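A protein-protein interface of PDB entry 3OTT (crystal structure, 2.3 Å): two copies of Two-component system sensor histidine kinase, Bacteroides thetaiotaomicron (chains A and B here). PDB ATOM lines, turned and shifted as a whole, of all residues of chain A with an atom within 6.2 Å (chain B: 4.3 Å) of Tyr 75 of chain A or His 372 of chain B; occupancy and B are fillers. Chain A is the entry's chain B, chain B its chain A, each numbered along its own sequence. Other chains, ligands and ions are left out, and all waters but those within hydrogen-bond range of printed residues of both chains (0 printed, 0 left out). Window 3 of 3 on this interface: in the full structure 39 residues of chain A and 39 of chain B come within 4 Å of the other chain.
The side-chain hydroxyl (OH) of Tyr 75 of chain A sits at hydrogen-bond distance from a ring nitrogen (NE2) of His 372 of chain B (2.7 Å).
ND2 of Asn 373 of chain B sits at hydrogen-bond distance from O of Asp 72 of chain A (3.4 Å).
NH2 of Arg 374 of chain B is in salt-bridge range of OD1 of Asp 72 of chain A, at 2.7 Å.
The guanidinium group (NH1) of Arg 131 of chain A lies within salt-bridge range of the side-chain carboxylate (OD2) of Asp 391 of chain B (3.4 Å).
ND1 of His 372 of chain B lies within hydrogen-bond range of N of Arg 374 of chain B.
O of Arg 374 of chain B sits at hydrogen-bond distance from N of Asp 391 of chain B (3.2 Å).
OH of Tyr 89 of chain A is in hydrogen-bond range of O of Asn 73 of chain A (3.1 Å).
Among the printed residues, merely in contact across the chains: Asp 72 of chain A with His 372 of chain B and Asn 73 of chain A with Asn 373 of chain B.
Of the printed residues of chain B, Asp 72 of chain A touches His 372, Asn 373 and Arg 374.
Of chain B, only His 372 comes within 4 Å of Tyr 75 of chain A.
His 372 of chain B touches two residues of chain A.
Printed residues of chain A within 4 Å of Arg 374 of chain B: Asp 72 (2.7 Å).
Of the printed residues of chain A, Asp 391 of chain B touches Arg 131 (3.4 Å).
Of the 8 printed residues of chain B, 4 touch a printed residue of chain A.
Hydrophobic or aromatic side chains of chain B within 4 Å of the printed part of chain A: His 372.
Along chain B the printed residues that touch a printed residue of chain A span positions 372 to 391.
Printed residues of chain A that touch a printed residue of chain B: Asp 72, Asn 73, Tyr 75 and Arg 131.
Among the printed residues, 6 pairs touch across the chains.
Among the printed residues, Asp or Glu carboxylates within 4 Å of a Lys or Arg side-chain nitrogen of the other chain: Asp 72 of chain A with Arg 374 of chain B (2.7 Å) and Arg 131 of chain A with Asp 391 of chain B (3.4 Å).
No position is printed for both chains.
Of the 6 pairs that touch across the chains among the printed residues, none has its exchanged pair printed and touching as well.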
ATOM      1  N   VAL A  69     -10.052   1.045  31.693  1.00  0.00           N
ATOM      2  CA  VAL A  69      -8.718   1.531  31.959  1.00  0.00           C
ATOM      3  C   VAL A  69      -8.648   3.020  31.654  1.00  0.00           C
ATOM      4  O   VAL A  69      -9.439   3.516  30.861  1.00  0.00           O
ATOM      5  CB  VAL A  69      -7.599   0.873  31.083  1.00  0.00           C
ATOM      6  CG1 VAL A  69      -7.333  -0.475  31.552  1.00  0.00           C
ATOM      7  CG2 VAL A  69      -7.924   0.915  29.609  1.00  0.00           C
ATOM      8  N   ILE A  70      -7.683   3.706  32.262  1.00  0.00           N
ATOM      9  CA  ILE A  70      -7.467   5.109  32.001  1.00  0.00           C
ATOM     10  C   ILE A  70      -6.404   5.227  30.880  1.00  0.00           C
ATOM     11  O   ILE A  70      -5.336   4.600  30.980  1.00  0.00           O
ATOM     12  CB  ILE A  70      -7.024   5.819  33.294  1.00  0.00           C
ATOM     13  CG1 ILE A  70      -8.167   5.788  34.328  1.00  0.00           C
ATOM     14  CG2 ILE A  70      -6.547   7.240  33.009  1.00  0.00           C
ATOM     15  CD1 ILE A  70      -7.820   6.508  35.686  1.00  0.00           C
ATOM     16  N   ILE A  71      -6.693   6.068  29.874  1.00  0.00           N
ATOM     17  CA  ILE A  71      -5.860   6.283  28.704  1.00  0.00           C
ATOM     18  C   ILE A  71      -5.491   7.789  28.577  1.00  0.00           C
ATOM     19  O   ILE A  71      -6.330   8.665  28.778  1.00  0.00           O
ATOM     20  CB  ILE A  71      -6.639   5.799  27.395  1.00  0.00           C
ATOM     21  CG1 ILE A  71      -6.906   4.283  27.378  1.00  0.00           C
ATOM     22  CG2 ILE A  71      -5.988   6.225  26.133  1.00  0.00           C
ATOM     23  CD1 ILE A  71      -5.712   3.435  27.630  1.00  0.00           C
ATOM     24  N   ASP A  72      -4.226   8.072  28.271  1.00  0.00           N
ATOM     25  CA  ASP A  72      -3.698   9.442  28.050  1.00  0.00           C
ATOM     26  C   ASP A  72      -3.958  10.415  29.217  1.00  0.00           C
ATOM     27  O   ASP A  72      -4.010  11.601  29.003  1.00  0.00           O
ATOM     28  CB  ASP A  72      -4.172  10.037  26.691  1.00  0.00           C
ATOM     29  CG  ASP A  72      -3.762   9.163  25.458  1.00  0.00           C
ATOM     30  OD1 ASP A  72      -2.887   8.257  25.623  1.00  0.00           O
ATOM     31  OD2 ASP A  72      -4.313   9.389  24.331  1.00  0.00           O
ATOM     32  N   ASN A  73      -4.122   9.891  30.437  1.00  0.00           N
ATOM     33  CA  ASN A  73      -4.342  10.728  31.620  1.00  0.00           C
ATOM     34  C   ASN A  73      -5.588  11.622  31.415  1.00  0.00           C
ATOM     35  O   ASN A  73      -5.659  12.741  31.940  1.00  0.00           O
ATOM     36  CB  ASN A  73      -3.112  11.615  31.827  1.00  0.00           C
ATOM     37  CG  ASN A  73      -2.957  12.108  33.272  1.00  0.00           C
ATOM     38  OD1 ASN A  73      -3.471  11.523  34.231  1.00  0.00           O
ATOM     39  ND2 ASN A  73      -2.230  13.207  33.424  1.00  0.00           N
ATOM     40  N   THR A  74      -6.532  11.177  30.579  1.00  0.00           N
ATOM     41  CA  THR A  74      -7.713  11.967  30.371  1.00  0.00           C
ATOM     42  C   THR A  74      -8.961  11.184  30.013  1.00  0.00           C
ATOM     43  O   THR A  74     -10.053  11.734  30.133  1.00  0.00           O
ATOM     44  CB  THR A  74      -7.502  13.157  29.385  1.00  0.00           C
ATOM     45  OG1 THR A  74      -8.632  14.027  29.467  1.00  0.00           O
ATOM     46  CG2 THR A  74      -7.345  12.709  27.916  1.00  0.00           C
ATOM     47  N   TYR A  75      -8.834   9.931  29.556  1.00  0.00           N
ATOM     48  CA  TYR A  75     -10.047   9.151  29.171  1.00  0.00           C
ATOM     49  C   TYR A  75     -10.309   7.949  30.067  1.00  0.00           C
ATOM     50  O   TYR A  75      -9.398   7.327  30.587  1.00  0.00           O
ATOM     51  CB  TYR A  75      -9.994   8.638  27.715  1.00  0.00           C
ATOM     52  CG  TYR A  75      -9.656   9.677  26.665  1.00  0.00           C
ATOM     53  CD1 TYR A  75     -10.612  10.626  26.233  1.00  0.00           C
ATOM     54  CD2 TYR A  75      -8.395   9.706  26.079  1.00  0.00           C
ATOM     55  CE1 TYR A  75     -10.278  11.599  25.284  1.00  0.00           C
ATOM     56  CE2 TYR A  75      -8.046  10.695  25.134  1.00  0.00           C
ATOM     57  CZ  TYR A  75      -8.982  11.617  24.747  1.00  0.00           C
ATOM     58  OH  TYR A  75      -8.583  12.522  23.779  1.00  0.00           O
ATOM     59  N   LEU A  76     -11.555   7.603  30.234  1.00  0.00           N
ATOM     60  CA  LEU A  76     -11.903   6.304  30.788  1.00  0.00           C
ATOM     61  C   LEU A  76     -12.432   5.513  29.606  1.00  0.00           C
ATOM     62  O   LEU A  76     -13.446   5.942  29.022  1.00  0.00           O
ATOM     63  CB  LEU A  76     -12.987   6.416  31.885  1.00  0.00           C
ATOM     64  CG  LEU A  76     -12.626   6.778  33.333  1.00  0.00           C
ATOM     65  CD1 LEU A  76     -11.395   7.626  33.478  1.00  0.00           C
ATOM     66  CD2 LEU A  76     -13.783   7.489  34.005  1.00  0.00           C
ATOM     67  N   TYR A  77     -11.695   4.477  29.189  1.00  0.00           N
ATOM     68  CA  TYR A  77     -12.141   3.500  28.196  1.00  0.00           C
ATOM     69  C   TYR A  77     -12.835   2.404  28.979  1.00  0.00           C
ATOM     70  O   TYR A  77     -12.233   1.773  29.859  1.00  0.00           O
ATOM     71  CB  TYR A  77     -10.932   2.881  27.392  1.00  0.00           C
ATOM     72  CG  TYR A  77     -10.448   3.703  26.213  1.00  0.00           C
ATOM     73  CD1 TYR A  77     -10.316   5.096  26.314  1.00  0.00           C
ATOM     74  CD2 TYR A  77     -10.101   3.088  25.014  1.00  0.00           C
ATOM     75  CE1 TYR A  77      -9.893   5.876  25.213  1.00  0.00           C
ATOM     76  CE2 TYR A  77      -9.637   3.813  23.913  1.00  0.00           C
ATOM     77  CZ  TYR A  77      -9.547   5.219  24.004  1.00  0.00           C
ATOM     78  OH  TYR A  77      -9.112   5.956  22.901  1.00  0.00           O
ATOM     79  N   VAL A  86     -16.090   5.661  25.569  1.00  0.00           N
ATOM     80  CA  VAL A  86     -14.982   6.501  25.924  1.00  0.00           C
ATOM     81  C   VAL A  86     -15.411   7.815  26.638  1.00  0.00           C
ATOM     82  O   VAL A  86     -16.112   8.669  26.057  1.00  0.00           O
ATOM     83  CB  VAL A  86     -14.112   6.785  24.705  1.00  0.00           C
ATOM     84  CG1 VAL A  86     -13.019   7.776  25.046  1.00  0.00           C
ATOM     85  CG2 VAL A  86     -13.514   5.470  24.182  1.00  0.00           C
ATOM     86  N   TYR A  87     -14.946   8.009  27.864  1.00  0.00           N
ATOM     87  CA  TYR A  87     -15.378   9.162  28.615  1.00  0.00           C
ATOM     88  C   TYR A  87     -14.193  10.080  28.897  1.00  0.00           C
ATOM     89  O   TYR A  87     -13.183   9.670  29.490  1.00  0.00           O
ATOM     90  CB  TYR A  87     -16.107   8.716  29.916  1.00  0.00           C
ATOM     91  CG  TYR A  87     -16.541   9.856  30.820  1.00  0.00           C
ATOM     92  CD1 TYR A  87     -17.630  10.705  30.467  1.00  0.00           C
ATOM     93  CD2 TYR A  87     -15.904  10.083  32.011  1.00  0.00           C
ATOM     94  CE1 TYR A  87     -18.030  11.769  31.298  1.00  0.00           C
ATOM     95  CE2 TYR A  87     -16.312  11.131  32.885  1.00  0.00           C
ATOM     96  CZ  TYR A  87     -17.360  11.953  32.507  1.00  0.00           C
ATOM     97  OH  TYR A  87     -17.730  12.949  33.353  1.00  0.00           O
ATOM     98  N   ASN A  88     -14.286  11.313  28.433  1.00  0.00           N
ATOM     99  CA  ASN A  88     -13.244  12.303  28.775  1.00  0.00           C
ATOM    100  C   ASN A  88     -13.553  12.895  30.143  1.00  0.00           C
ATOM    101  O   ASN A  88     -14.427  13.696  30.262  1.00  0.00           O
ATOM    102  CB  ASN A  88     -13.106  13.384  27.675  1.00  0.00           C
ATOM    103  CG  ASN A  88     -11.981  14.385  27.956  1.00  0.00           C
ATOM    104  OD1 ASN A  88     -11.573  14.562  29.096  1.00  0.00           O
ATOM    105  ND2 ASN A  88     -11.482  15.054  26.897  1.00  0.00           N
ATOM    106  N   TYR A  89     -12.835  12.493  31.174  1.00  0.00           N
ATOM    107  CA  TYR A  89     -13.208  12.910  32.499  1.00  0.00           C
ATOM    108  C   TYR A  89     -12.760  14.355  32.827  1.00  0.00           C
ATOM    109  O   TYR A  89     -13.271  14.975  33.782  1.00  0.00           O
ATOM    110  CB  TYR A  89     -12.696  11.890  33.525  1.00  0.00           C
ATOM    111  CG  TYR A  89     -11.186  11.919  33.801  1.00  0.00           C
ATOM    112  CD1 TYR A  89     -10.616  12.864  34.656  1.00  0.00           C
ATOM    113  CD2 TYR A  89     -10.338  10.993  33.191  1.00  0.00           C
ATOM    114  CE1 TYR A  89      -9.235  12.853  34.940  1.00  0.00           C
ATOM    115  CE2 TYR A  89      -8.943  10.977  33.454  1.00  0.00           C
ATOM    116  CZ  TYR A  89      -8.408  11.908  34.291  1.00  0.00           C
ATOM    117  OH  TYR A  89      -7.068  11.856  34.523  1.00  0.00           O
ATOM    118  N   GLU A  95     -16.632  10.970  24.207  1.00  0.00           N
ATOM    119  CA  GLU A  95     -15.882  11.391  23.046  1.00  0.00           C
ATOM    120  C   GLU A  95     -15.517  10.202  22.264  1.00  0.00           C
ATOM    121  O   GLU A  95     -14.399   9.727  22.471  1.00  0.00           O
ATOM    122  CB  GLU A  95     -14.561  12.103  23.465  1.00  0.00           C
ATOM    123  CG  GLU A  95     -14.760  13.641  23.507  1.00  0.00           C
ATOM    124  CD  GLU A  95     -13.575  14.446  24.049  1.00  0.00           C
ATOM    125  OE1 GLU A  95     -12.445  13.912  24.032  1.00  0.00           O
ATOM    126  OE2 GLU A  95     -13.790  15.638  24.456  1.00  0.00           O
ATOM    127  N   ARG A 131      -4.338   3.995  15.738  1.00  0.00           N
ATOM    128  CA  ARG A 131      -5.731   3.569  15.825  1.00  0.00           C
ATOM    129  C   ARG A 131      -6.004   2.238  15.043  1.00  0.00           C
ATOM    130  O   ARG A 131      -7.137   1.947  14.616  1.00  0.00           O
ATOM    131  CB  ARG A 131      -6.691   4.755  15.492  1.00  0.00           C
ATOM    132  CG  ARG A 131      -6.534   6.001  16.488  1.00  0.00           C
ATOM    133  CD  ARG A 131      -7.593   7.206  16.328  1.00  0.00           C
ATOM    134  NE  ARG A 131      -8.052   7.724  17.653  1.00  0.00           N
ATOM    135  CZ  ARG A 131      -7.795   8.939  18.209  1.00  0.00           C
ATOM    136  NH1 ARG A 131      -7.086   9.892  17.568  1.00  0.00           N
ATOM    137  NH2 ARG A 131      -8.289   9.218  19.433  1.00  0.00           N
ATOM    138  N   LEU B 370      -0.040  21.288  28.386  1.00  0.00           N
ATOM    139  CA  LEU B 370      -0.501  21.096  27.016  1.00  0.00           C
ATOM    140  C   LEU B 370      -1.968  20.785  27.029  1.00  0.00           C
ATOM    141  O   LEU B 370      -2.459  20.186  27.990  1.00  0.00           O
ATOM    142  CB  LEU B 370       0.229  19.921  26.354  1.00  0.00           C
ATOM    143  CG  LEU B 370       1.540  20.233  25.685  1.00  0.00           C
ATOM    144  CD1 LEU B 370       2.000  19.017  24.913  1.00  0.00           C
ATOM    145  CD2 LEU B 370       1.434  21.461  24.754  1.00  0.00           C
ATOM    146  N   SER B 371      -2.673  21.166  25.974  1.00  0.00           N
ATOM    147  CA  SER B 371      -4.090  20.797  25.852  1.00  0.00           C
ATOM    148  C   SER B 371      -4.284  19.263  25.870  1.00  0.00           C
ATOM    149  O   SER B 371      -5.280  18.821  26.364  1.00  0.00           O
ATOM    150  CB  SER B 371      -4.738  21.391  24.604  1.00  0.00           C
ATOM    151  OG  SER B 371      -4.028  20.930  23.458  1.00  0.00           O
ATOM    152  N   HIS B 372      -3.304  18.481  25.409  1.00  0.00           N
ATOM    153  CA  HIS B 372      -3.411  16.988  25.289  1.00  0.00           C
ATOM    154  C   HIS B 372      -2.022  16.388  25.225  1.00  0.00           C
ATOM    155  O   HIS B 372      -1.110  16.995  24.664  1.00  0.00           O
ATOM    156  CB  HIS B 372      -4.171  16.600  24.007  1.00  0.00           C
ATOM    157  CG  HIS B 372      -4.764  15.217  24.014  1.00  0.00           C
ATOM    158  ND1 HIS B 372      -4.003  14.070  23.891  1.00  0.00           N
ATOM    159  CD2 HIS B 372      -6.058  14.803  24.085  1.00  0.00           C
ATOM    160  CE1 HIS B 372      -4.803  13.010  23.907  1.00  0.00           C
ATOM    161  NE2 HIS B 372      -6.053  13.426  24.033  1.00  0.00           N
ATOM    162  N   ASN B 373      -1.851  15.182  25.754  1.00  0.00           N
ATOM    163  CA  ASN B 373      -0.539  14.558  25.834  1.00  0.00           C
ATOM    164  C   ASN B 373      -0.058  13.991  24.496  1.00  0.00           C
ATOM    165  O   ASN B 373       1.157  13.901  24.236  1.00  0.00           O
ATOM    166  CB  ASN B 373      -0.578  13.431  26.841  1.00  0.00           C
ATOM    167  CG  ASN B 373      -0.414  13.901  28.284  1.00  0.00           C
ATOM    168  OD1 ASN B 373       0.205  14.914  28.559  1.00  0.00           O
ATOM    169  ND2 ASN B 373      -0.939  13.121  29.211  1.00  0.00           N
ATOM    170  N   ARG B 374      -0.999  13.597  23.643  1.00  0.00           N
ATOM    171  CA  ARG B 374      -0.663  12.740  22.496  1.00  0.00           C
ATOM    172  C   ARG B 374      -0.219  13.636  21.334  1.00  0.00           C
ATOM    173  O   ARG B 374      -1.038  14.240  20.651  1.00  0.00           O
ATOM    174  CB  ARG B 374      -1.890  11.868  22.119  1.00  0.00           C
ATOM    175  CG  ARG B 374      -1.656  10.757  21.119  1.00  0.00           C
ATOM    176  CD  ARG B 374      -2.749   9.636  21.101  1.00  0.00           C
ATOM    177  NE  ARG B 374      -2.593   8.751  22.259  1.00  0.00           N
ATOM    178  CZ  ARG B 374      -1.602   7.851  22.408  1.00  0.00           C
ATOM    179  NH1 ARG B 374      -0.621   7.669  21.477  1.00  0.00           N
ATOM    180  NH2 ARG B 374      -1.567   7.166  23.509  1.00  0.00           N
ATOM    181  N   ASP B 391      -3.855  15.643  19.872  1.00  0.00           N
ATOM    182  CA  ASP B 391      -5.279  15.310  20.010  1.00  0.00           C
ATOM    183  C   ASP B 391      -6.075  16.355  20.856  1.00  0.00           C
ATOM    184  O   ASP B 391      -7.201  16.114  21.245  1.00  0.00           O
ATOM    185  CB  ASP B 391      -5.431  13.864  20.551  1.00  0.00           C
ATOM    186  CG  ASP B 391      -5.281  12.788  19.451  1.00  0.00           C
ATOM    187  OD1 ASP B 391      -5.318  13.130  18.246  1.00  0.00           O
ATOM    188  OD2 ASP B 391      -5.153  11.573  19.787  1.00  0.00           O
ATOM    189  N   GLY B 392      -5.438  17.495  21.164  1.00  0.00           N
ATOM    190  CA  GLY B 392      -6.118  18.683  21.655  1.00  0.00           C
ATOM    191  C   GLY B 392      -5.750  19.855  20.749  1.00  0.00           C
ATOM    192  O   GLY B 392      -5.211  20.871  21.206  1.00  0.00           O
ATOM    193  N   TRP B 420      -8.722  16.746  16.769  1.00  0.00           N
ATOM    194  CA  TRP B 420      -7.773  15.663  16.518  1.00  0.00           C
ATOM    195  C   TRP B 420      -6.960  15.936  15.255  1.00  0.00           C
ATOM    196  O   TRP B 420      -7.342  15.531  14.142  1.00  0.00           O
ATOM    197  CB  TRP B 420      -8.466  14.298  16.480  1.00  0.00           C
ATOM    198  CG  TRP B 420      -9.214  13.972  17.774  1.00  0.00           C
ATOM    199  CD1 TRP B 420      -8.913  14.420  19.047  1.00  0.00           C
ATOM    200  CD2 TRP B 420     -10.390  13.162  17.912  1.00  0.00           C
ATOM    201  NE1 TRP B 420      -9.823  13.929  19.952  1.00  0.00           N
ATOM    202  CE2 TRP B 420     -10.735  13.150  19.289  1.00  0.00           C
ATOM    203  CE3 TRP B 420     -11.189  12.438  17.006  1.00  0.00           C
ATOM    204  CZ2 TRP B 420     -11.850  12.428  19.787  1.00  0.00           C
ATOM    205  CZ3 TRP B 420     -12.305  11.717  17.502  1.00  0.00           C
ATOM    206  CH2 TRP B 420     -12.618  11.723  18.881  1.00  0.00           C
